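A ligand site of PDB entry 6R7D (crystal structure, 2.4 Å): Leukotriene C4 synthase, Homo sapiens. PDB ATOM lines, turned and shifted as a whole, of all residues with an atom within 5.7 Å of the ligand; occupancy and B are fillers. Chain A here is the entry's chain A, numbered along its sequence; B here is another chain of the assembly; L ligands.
NH2 of Arg 97 lies within hydrogen-bond range of O3 of the ligand (2.9 Å).
OH of Tyr 66 lies within hydrogen-bond range of N2 of the ligand.
The side-chain hydroxyl of Tyr 100 is in hydrogen-bond range of an oxygen (O1) of the ligand.
The guanidinium group (NE) of Arg 111 lies within salt-bridge range of an oxygen (O1) of the ligand, 2.7 Å away.
OD1 of Asn 62 touches C12 of the ligand, 3.5 Å away.
Leu 69 touches the ligand.
Tyr 104 touches the ligand (CE2 to O1, 3.9 Å).
Leu 115 touches the ligand.
O of Ser 118 touches C14 of the ligand, 3.9 Å away.
Ala 119 touches the ligand.
Leu 122 touches the ligand.
Trp 123 touches the ligand (NE1 to C5, 3.5 Å).
Val 23 of chain B touches the ligand.
Gln 26 of chain B touches the ligand.
Ala 27 of chain B touches the ligand (CA to C1, 3.3 Å).
Ser 30 of chain B touches the ligand.
Hydrophobic or aromatic side chains within 4 Å of the ligand: Tyr 66, Leu 69, Tyr 100, Tyr 104, Leu 115, Ala 119, Leu 122, Trp 123 and Ala 27 of chain B.
The side-chain hydroxyl (OG) of Ser 30 of chain B lies within hydrogen-bond range of the backbone carbonyl oxygen (O) of Gln 26 of chain B (3.4 Å).
OH of Tyr 100 sits at hydrogen-bond distance from OD1 of Asn 62 (3.0 Å).
The guanidinium group (NE) of Arg 97 is in hydrogen-bond range of the side-chain hydroxyl (OH) of Tyr 93.
The side-chain hydroxyl of Ser 30 of chain B lies within hydrogen-bond range of the side-chain hydroxyl of Tyr 66, 3.0 Å away.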
ATOM      1  N   ASN A  62      11.708 -25.538  16.336  1.00  0.00           N
ATOM      2  CA  ASN A  62      11.000 -26.210  15.248  1.00  0.00           C
ATOM      3  C   ASN A  62      11.997 -26.289  14.085  1.00  0.00           C
ATOM      4  O   ASN A  62      12.091 -27.336  13.467  1.00  0.00           O
ATOM      5  CB  ASN A  62       9.748 -25.519  14.840  1.00  0.00           C
ATOM      6  CG  ASN A  62       8.634 -25.561  15.963  1.00  0.00           C
ATOM      7  OD1 ASN A  62       7.843 -24.597  16.097  1.00  0.00           O
ATOM      8  ND2 ASN A  62       8.566 -26.608  16.681  1.00  0.00           N
ATOM      9  N   TYR A  66      13.362 -29.987  12.337  1.00  0.00           N
ATOM     10  CA  TYR A  66      13.168 -30.321  10.979  1.00  0.00           C
ATOM     11  C   TYR A  66      14.481 -30.318  10.197  1.00  0.00           C
ATOM     12  O   TYR A  66      14.542 -30.915   9.106  1.00  0.00           O
ATOM     13  CB  TYR A  66      12.147 -29.358  10.334  1.00  0.00           C
ATOM     14  CG  TYR A  66      10.772 -29.717  10.692  1.00  0.00           C
ATOM     15  CD1 TYR A  66      10.228 -29.347  11.902  1.00  0.00           C
ATOM     16  CD2 TYR A  66      10.003 -30.576   9.866  1.00  0.00           C
ATOM     17  CE1 TYR A  66       8.948 -29.677  12.249  1.00  0.00           C
ATOM     18  CE2 TYR A  66       8.716 -31.004  10.285  1.00  0.00           C
ATOM     19  CZ  TYR A  66       8.169 -30.529  11.411  1.00  0.00           C
ATOM     20  OH  TYR A  66       6.875 -30.870  11.822  1.00  0.00           O
ATOM     21  N   LEU A  69      15.566 -33.675   8.771  1.00  0.00           N
ATOM     22  CA  LEU A  69      14.651 -34.116   7.761  1.00  0.00           C
ATOM     23  C   LEU A  69      14.904 -33.464   6.440  1.00  0.00           C
ATOM     24  O   LEU A  69      14.905 -34.118   5.446  1.00  0.00           O
ATOM     25  CB  LEU A  69      13.189 -33.849   8.136  1.00  0.00           C
ATOM     26  CG  LEU A  69      12.699 -34.429   9.505  1.00  0.00           C
ATOM     27  CD1 LEU A  69      11.236 -34.149   9.772  1.00  0.00           C
ATOM     28  CD2 LEU A  69      12.987 -35.882   9.612  1.00  0.00           C
ATOM     29  N   TYR A  93      13.516 -24.045   0.677  1.00  0.00           N
ATOM     30  CA  TYR A  93      13.221 -24.477   2.024  1.00  0.00           C
ATOM     31  C   TYR A  93      13.891 -23.545   3.106  1.00  0.00           C
ATOM     32  O   TYR A  93      13.213 -23.028   4.023  1.00  0.00           O
ATOM     33  CB  TYR A  93      13.595 -25.948   2.269  1.00  0.00           C
ATOM     34  CG  TYR A  93      13.394 -26.408   3.667  1.00  0.00           C
ATOM     35  CD1 TYR A  93      12.115 -26.715   4.149  1.00  0.00           C
ATOM     36  CD2 TYR A  93      14.421 -26.381   4.574  1.00  0.00           C
ATOM     37  CE1 TYR A  93      11.884 -27.021   5.512  1.00  0.00           C
ATOM     38  CE2 TYR A  93      14.198 -26.680   5.909  1.00  0.00           C
ATOM     39  CZ  TYR A  93      12.917 -26.991   6.382  1.00  0.00           C
ATOM     40  OH  TYR A  93      12.741 -27.279   7.748  1.00  0.00           O
ATOM     41  N   ARG A  97      12.269 -20.888   5.765  1.00  0.00           N
ATOM     42  CA  ARG A  97      12.418 -20.990   7.188  1.00  0.00           C
ATOM     43  C   ARG A  97      12.928 -19.750   7.801  1.00  0.00           C
ATOM     44  O   ARG A  97      12.552 -19.431   8.945  1.00  0.00           O
ATOM     45  CB  ARG A  97      13.372 -22.149   7.568  1.00  0.00           C
ATOM     46  CG  ARG A  97      12.723 -23.546   7.456  1.00  0.00           C
ATOM     47  CD  ARG A  97      11.506 -23.600   8.424  1.00  0.00           C
ATOM     48  NE  ARG A  97      11.081 -24.897   8.579  1.00  0.00           N
ATOM     49  CZ  ARG A  97      10.134 -25.338   9.375  1.00  0.00           C
ATOM     50  NH1 ARG A  97       9.423 -24.536  10.047  1.00  0.00           N
ATOM     51  NH2 ARG A  97       9.976 -26.620   9.525  1.00  0.00           N
ATOM     52  N   TYR A 100       9.916 -17.804   8.050  1.00  0.00           N
ATOM     53  CA  TYR A 100       9.091 -18.376   9.099  1.00  0.00           C
ATOM     54  C   TYR A 100       9.531 -17.933  10.479  1.00  0.00           C
ATOM     55  O   TYR A 100       8.723 -17.504  11.285  1.00  0.00           O
ATOM     56  CB  TYR A 100       9.152 -19.838   9.031  1.00  0.00           C
ATOM     57  CG  TYR A 100       8.759 -20.571  10.319  1.00  0.00           C
ATOM     58  CD1 TYR A 100       7.404 -20.794  10.662  1.00  0.00           C
ATOM     59  CD2 TYR A 100       9.746 -21.142  11.152  1.00  0.00           C
ATOM     60  CE1 TYR A 100       7.065 -21.506  11.782  1.00  0.00           C
ATOM     61  CE2 TYR A 100       9.409 -21.817  12.322  1.00  0.00           C
ATOM     62  CZ  TYR A 100       8.079 -22.044  12.617  1.00  0.00           C
ATOM     63  OH  TYR A 100       7.707 -22.733  13.777  1.00  0.00           O
ATOM     64  N   TYR A 104       7.328 -15.602  12.931  1.00  0.00           N
ATOM     65  CA  TYR A 104       6.953 -16.139  14.187  1.00  0.00           C
ATOM     66  C   TYR A 104       7.421 -15.204  15.366  1.00  0.00           C
ATOM     67  O   TYR A 104       6.602 -14.949  16.248  1.00  0.00           O
ATOM     68  CB  TYR A 104       7.537 -17.519  14.435  1.00  0.00           C
ATOM     69  CG  TYR A 104       6.771 -18.460  15.392  1.00  0.00           C
ATOM     70  CD1 TYR A 104       5.697 -18.008  16.253  1.00  0.00           C
ATOM     71  CD2 TYR A 104       7.165 -19.768  15.497  1.00  0.00           C
ATOM     72  CE1 TYR A 104       5.110 -18.880  17.163  1.00  0.00           C
ATOM     73  CE2 TYR A 104       6.569 -20.611  16.371  1.00  0.00           C
ATOM     74  CZ  TYR A 104       5.494 -20.141  17.201  1.00  0.00           C
ATOM     75  OH  TYR A 104       4.921 -21.081  17.982  1.00  0.00           O
ATOM     76  N   ARG A 111       3.783 -16.303  11.175  1.00  0.00           N
ATOM     77  CA  ARG A 111       4.531 -17.402  10.878  1.00  0.00           C
ATOM     78  C   ARG A 111       3.845 -18.259   9.808  1.00  0.00           C
ATOM     79  O   ARG A 111       4.554 -19.092   9.163  1.00  0.00           O
ATOM     80  CB  ARG A 111       4.822 -18.273  12.104  1.00  0.00           C
ATOM     81  CG  ARG A 111       3.887 -19.479  12.309  1.00  0.00           C
ATOM     82  CD  ARG A 111       4.058 -19.952  13.761  1.00  0.00           C
ATOM     83  NE  ARG A 111       3.431 -21.219  13.977  1.00  0.00           N
ATOM     84  CZ  ARG A 111       2.112 -21.436  14.095  1.00  0.00           C
ATOM     85  NH1 ARG A 111       1.652 -22.681  14.232  1.00  0.00           N
ATOM     86  NH2 ARG A 111       1.269 -20.423  14.159  1.00  0.00           N
ATOM     87  N   LEU A 115       5.567 -20.743   6.976  1.00  0.00           N
ATOM     88  CA  LEU A 115       5.488 -22.127   7.408  1.00  0.00           C
ATOM     89  C   LEU A 115       4.948 -23.018   6.325  1.00  0.00           C
ATOM     90  O   LEU A 115       5.562 -24.054   6.013  1.00  0.00           O
ATOM     91  CB  LEU A 115       4.570 -22.274   8.609  1.00  0.00           C
ATOM     92  CG  LEU A 115       4.227 -23.699   9.104  1.00  0.00           C
ATOM     93  CD1 LEU A 115       5.498 -24.381   9.491  1.00  0.00           C
ATOM     94  CD2 LEU A 115       3.316 -23.706  10.337  1.00  0.00           C
ATOM     95  N   SER A 118       7.469 -23.458   3.687  1.00  0.00           N
ATOM     96  CA  SER A 118       8.487 -24.373   4.162  1.00  0.00           C
ATOM     97  C   SER A 118       8.017 -25.829   3.928  1.00  0.00           C
ATOM     98  O   SER A 118       8.816 -26.697   3.475  1.00  0.00           O
ATOM     99  CB  SER A 118       8.693 -24.315   5.665  1.00  0.00           C
ATOM    100  OG  SER A 118       9.326 -23.098   6.060  1.00  0.00           O
ATOM    101  N   ALA A 119       6.755 -26.063   4.202  1.00  0.00           N
ATOM    102  CA  ALA A 119       6.210 -27.392   4.092  1.00  0.00           C
ATOM    103  C   ALA A 119       6.085 -27.843   2.629  1.00  0.00           C
ATOM    104  O   ALA A 119       6.408 -28.971   2.321  1.00  0.00           O
ATOM    105  CB  ALA A 119       4.827 -27.448   4.801  1.00  0.00           C
ATOM    106  N   ARG A 120       5.681 -26.931   1.746  1.00  0.00           N
ATOM    107  CA  ARG A 120       5.642 -27.211   0.329  1.00  0.00           C
ATOM    108  C   ARG A 120       7.062 -27.563  -0.177  1.00  0.00           C
ATOM    109  O   ARG A 120       7.201 -28.542  -0.939  1.00  0.00           O
ATOM    110  CB  ARG A 120       5.026 -26.059  -0.525  1.00  0.00           C
ATOM    111  CG  ARG A 120       3.487 -26.012  -0.310  1.00  0.00           C
ATOM    112  CD  ARG A 120       2.730 -25.059  -1.208  1.00  0.00           C
ATOM    113  NE  ARG A 120       3.334 -23.699  -1.159  1.00  0.00           N
ATOM    114  CZ  ARG A 120       2.972 -22.692  -0.342  1.00  0.00           C
ATOM    115  NH1 ARG A 120       1.954 -22.798   0.497  1.00  0.00           N
ATOM    116  NH2 ARG A 120       3.647 -21.541  -0.421  1.00  0.00           N
ATOM    117  N   LEU A 122       9.643 -28.734   1.469  1.00  0.00           N
ATOM    118  CA  LEU A 122      10.033 -29.996   1.971  1.00  0.00           C
ATOM    119  C   LEU A 122       9.264 -31.161   1.318  1.00  0.00           C
ATOM    120  O   LEU A 122       9.882 -32.202   1.042  1.00  0.00           O
ATOM    121  CB  LEU A 122       9.859 -30.070   3.469  1.00  0.00           C
ATOM    122  CG  LEU A 122      10.429 -31.311   4.161  1.00  0.00           C
ATOM    123  CD1 LEU A 122      11.949 -31.556   3.820  1.00  0.00           C
ATOM    124  CD2 LEU A 122      10.254 -31.186   5.630  1.00  0.00           C
ATOM    125  N   TRP A 123       7.987 -30.982   0.984  1.00  0.00           N
ATOM    126  CA  TRP A 123       7.253 -31.995   0.239  1.00  0.00           C
ATOM    127  C   TRP A 123       7.813 -32.230  -1.188  1.00  0.00           C
ATOM    128  O   TRP A 123       7.815 -33.319  -1.664  1.00  0.00           O
ATOM    129  CB  TRP A 123       5.749 -31.653   0.088  1.00  0.00           C
ATOM    130  CG  TRP A 123       4.874 -32.061   1.249  1.00  0.00           C
ATOM    131  CD1 TRP A 123       4.026 -31.204   1.979  1.00  0.00           C
ATOM    132  CD2 TRP A 123       4.680 -33.384   1.822  1.00  0.00           C
ATOM    133  NE1 TRP A 123       3.341 -31.928   2.961  1.00  0.00           N
ATOM    134  CE2 TRP A 123       3.744 -33.248   2.911  1.00  0.00           C
ATOM    135  CE3 TRP A 123       5.239 -34.627   1.601  1.00  0.00           C
ATOM    136  CZ2 TRP A 123       3.338 -34.337   3.674  1.00  0.00           C
ATOM    137  CZ3 TRP A 123       4.879 -35.720   2.412  1.00  0.00           C
ATOM    138  CH2 TRP A 123       3.959 -35.564   3.432  1.00  0.00           C
ATOM    139  N   VAL A 126      10.732 -34.335  -0.729  1.00  0.00           N
ATOM    140  CA  VAL A 126      10.229 -35.722  -0.502  1.00  0.00           C
ATOM    141  C   VAL A 126       9.782 -36.408  -1.852  1.00  0.00           C
ATOM    142  O   VAL A 126      10.178 -37.498  -2.115  1.00  0.00           O
ATOM    143  CB  VAL A 126       9.066 -35.784   0.504  1.00  0.00           C
ATOM    144  CG1 VAL A 126       8.400 -37.137   0.521  1.00  0.00           C
ATOM    145  CG2 VAL A 126       9.601 -35.435   1.875  1.00  0.00           C
ATOM    146  N   VAL B  23      11.448 -40.337   7.148  1.00  0.00           N
ATOM    147  CA  VAL B  23      10.948 -39.035   6.944  1.00  0.00           C
ATOM    148  C   VAL B  23       9.447 -39.024   6.852  1.00  0.00           C
ATOM    149  O   VAL B  23       8.773 -38.197   7.538  1.00  0.00           O
ATOM    150  CB  VAL B  23      11.575 -38.322   5.753  1.00  0.00           C
ATOM    151  CG1 VAL B  23      10.953 -36.973   5.483  1.00  0.00           C
ATOM    152  CG2 VAL B  23      13.083 -38.128   6.026  1.00  0.00           C
ATOM    153  N   GLN B  26       7.883 -39.544  10.281  1.00  0.00           N
ATOM    154  CA  GLN B  26       7.859 -38.277  10.992  1.00  0.00           C
ATOM    155  C   GLN B  26       6.749 -37.383  10.547  1.00  0.00           C
ATOM    156  O   GLN B  26       6.150 -36.703  11.379  1.00  0.00           O
ATOM    157  CB  GLN B  26       9.167 -37.495  10.917  1.00  0.00           C
ATOM    158  CG  GLN B  26      10.323 -38.204  11.647  1.00  0.00           C
ATOM    159  CD  GLN B  26      10.127 -38.451  13.133  1.00  0.00           C
ATOM    160  OE1 GLN B  26      10.502 -39.507  13.639  1.00  0.00           O
ATOM    161  NE2 GLN B  26       9.576 -37.463  13.850  1.00  0.00           N
ATOM    162  N   ALA B  27       6.472 -37.349   9.252  1.00  0.00           N
ATOM    163  CA  ALA B  27       5.332 -36.587   8.741  1.00  0.00           C
ATOM    164  C   ALA B  27       3.984 -37.025   9.347  1.00  0.00           C
ATOM    165  O   ALA B  27       3.154 -36.193   9.678  1.00  0.00           O
ATOM    166  CB  ALA B  27       5.267 -36.645   7.221  1.00  0.00           C
ATOM    167  N   TYR B  28       3.795 -38.326   9.433  1.00  0.00           N
ATOM    168  CA  TYR B  28       2.640 -38.915  10.072  1.00  0.00           C
ATOM    169  C   TYR B  28       2.560 -38.492  11.568  1.00  0.00           C
ATOM    170  O   TYR B  28       1.530 -38.047  12.050  1.00  0.00           O
ATOM    171  CB  TYR B  28       2.663 -40.476   9.913  1.00  0.00           C
ATOM    172  CG  TYR B  28       1.566 -41.118  10.679  1.00  0.00           C
ATOM    173  CD1 TYR B  28       0.241 -41.091  10.170  1.00  0.00           C
ATOM    174  CD2 TYR B  28       1.796 -41.694  11.920  1.00  0.00           C
ATOM    175  CE1 TYR B  28      -0.788 -41.655  10.884  1.00  0.00           C
ATOM    176  CE2 TYR B  28       0.782 -42.292  12.637  1.00  0.00           C
ATOM    177  CZ  TYR B  28      -0.509 -42.252  12.137  1.00  0.00           C
ATOM    178  OH  TYR B  28      -1.530 -42.803  12.900  1.00  0.00           O
ATOM    179  N   SER B  30       3.872 -35.711  12.916  1.00  0.00           N
ATOM    180  CA  SER B  30       3.501 -34.310  12.954  1.00  0.00           C
ATOM    181  C   SER B  30       2.061 -34.039  12.677  1.00  0.00           C
ATOM    182  O   SER B  30       1.480 -33.183  13.330  1.00  0.00           O
ATOM    183  CB  SER B  30       4.226 -33.462  11.960  1.00  0.00           C
ATOM    184  OG  SER B  30       5.571 -33.548  12.380  1.00  0.00           O
ATOM    185  N   LEU B  31       1.543 -34.782  11.732  1.00  0.00           N
ATOM    186  CA  LEU B  31       0.129 -34.743  11.405  1.00  0.00           C
ATOM    187  C   LEU B  31      -0.720 -35.069  12.668  1.00  0.00           C
ATOM    188  O   LEU B  31      -1.678 -34.352  12.945  1.00  0.00           O
ATOM    189  CB  LEU B  31      -0.188 -35.708  10.244  1.00  0.00           C
ATOM    190  CG  LEU B  31      -1.642 -35.705   9.638  1.00  0.00           C
ATOM    191  CD1 LEU B  31      -1.932 -34.361   9.007  1.00  0.00           C
ATOM    192  CD2 LEU B  31      -1.774 -36.809   8.597  1.00  0.00           C
ATOM    193  N   ILE B  34      -0.615 -32.129  15.025  1.00  0.00           N
ATOM    194  CA  ILE B  34      -1.466 -31.025  14.559  1.00  0.00           C
ATOM    195  C   ILE B  34      -2.943 -31.317  14.917  1.00  0.00           C
ATOM    196  O   ILE B  34      -3.691 -30.488  15.413  1.00  0.00           O
ATOM    197  CB  ILE B  34      -1.363 -30.816  13.044  1.00  0.00           C
ATOM    198  CG1 ILE B  34      -0.070 -30.080  12.746  1.00  0.00           C
ATOM    199  CG2 ILE B  34      -2.504 -29.927  12.517  1.00  0.00           C
ATOM    200  CD1 ILE B  34       0.403 -30.205  11.294  1.00  0.00           C
ATOM    201  N   PRO B  44       0.098 -23.096  19.328  1.00  0.00           N
ATOM    202  CA  PRO B  44       1.442 -22.623  19.386  1.00  0.00           C
ATOM    203  C   PRO B  44       1.544 -21.161  19.862  1.00  0.00           C
ATOM    204  O   PRO B  44       0.735 -20.418  19.406  1.00  0.00           O
ATOM    205  CB  PRO B  44       1.878 -22.737  17.948  1.00  0.00           C
ATOM    206  CG  PRO B  44       1.070 -23.913  17.399  1.00  0.00           C
ATOM    207  CD  PRO B  44      -0.277 -23.626  18.012  1.00  0.00           C
HETATM  208  C1  LIG L   1       7.269 -33.890   8.903  1.00  0.00           C
HETATM  209  C2  LIG L   1       8.070 -34.627   8.045  1.00  0.00           C
HETATM  210  C3  LIG L   1       8.129 -34.319   6.694  1.00  0.00           C
HETATM  211  C4  LIG L   1       5.870 -31.438   6.545  1.00  0.00           C
HETATM  212  C5  LIG L   1       5.964 -31.145   5.172  1.00  0.00           C
HETATM  213  C6  LIG L   1       6.749 -31.916   4.311  1.00  0.00           C
HETATM  214  C7  LIG L   1       7.467 -32.988   4.811  1.00  0.00           C
HETATM  215  C8  LIG L   1       5.399 -29.753   8.446  1.00  0.00           C
HETATM  216  C9  LIG L   1       4.681 -29.620   9.639  1.00  0.00           C
HETATM  217  C10 LIG L   1       6.096 -28.023  10.389  1.00  0.00           C
HETATM  218  C11 LIG L   1       6.525 -27.083  11.414  1.00  0.00           C
HETATM  219  C12 LIG L   1       5.900 -25.503  13.364  1.00  0.00           C
HETATM  220  C13 LIG L   1       4.912 -24.404  13.699  1.00  0.00           C
HETATM  221  C14 LIG L   1       8.337 -28.165   7.063  1.00  0.00           C
HETATM  222  C15 LIG L   1       1.800 -32.709   7.429  1.00  0.00           C
HETATM  223  C16 LIG L   1       3.098 -33.336   7.796  1.00  0.00           C
HETATM  224  C17 LIG L   1       7.404 -33.268   6.172  1.00  0.00           C
HETATM  225  C18 LIG L   1       6.611 -32.501   7.047  1.00  0.00           C
HETATM  226  C19 LIG L   1       6.538 -32.824   8.386  1.00  0.00           C
HETATM  227  N1  LIG L   1       5.036 -30.672   7.430  1.00  0.00           N
HETATM  228  N2  LIG L   1       5.000 -28.757  10.623  1.00  0.00           N
HETATM  229  C20 LIG L   1       5.553 -26.669  12.488  1.00  0.00           C
HETATM  230  C21 LIG L   1       5.809 -26.902  13.964  1.00  0.00           C
HETATM  231  O1  LIG L   1       5.232 -23.210  13.830  1.00  0.00           O
HETATM  232  O2  LIG L   1       3.652 -24.875  13.906  1.00  0.00           O
HETATM  233  O3  LIG L   1       7.685 -26.648  11.358  1.00  0.00           O
HETATM  234  N3  LIG L   1       6.878 -28.034   9.293  1.00  0.00           N
HETATM  235  C22 LIG L   1       6.509 -28.924   8.355  1.00  0.00           C
HETATM  236  O4  LIG L   1       7.232 -29.062   7.198  1.00  0.00           O
HETATM  237  C23 LIG L   1       3.602 -30.833   7.126  1.00  0.00           C
HETATM  238  C24 LIG L   1       2.929 -31.859   7.959  1.00  0.00           C
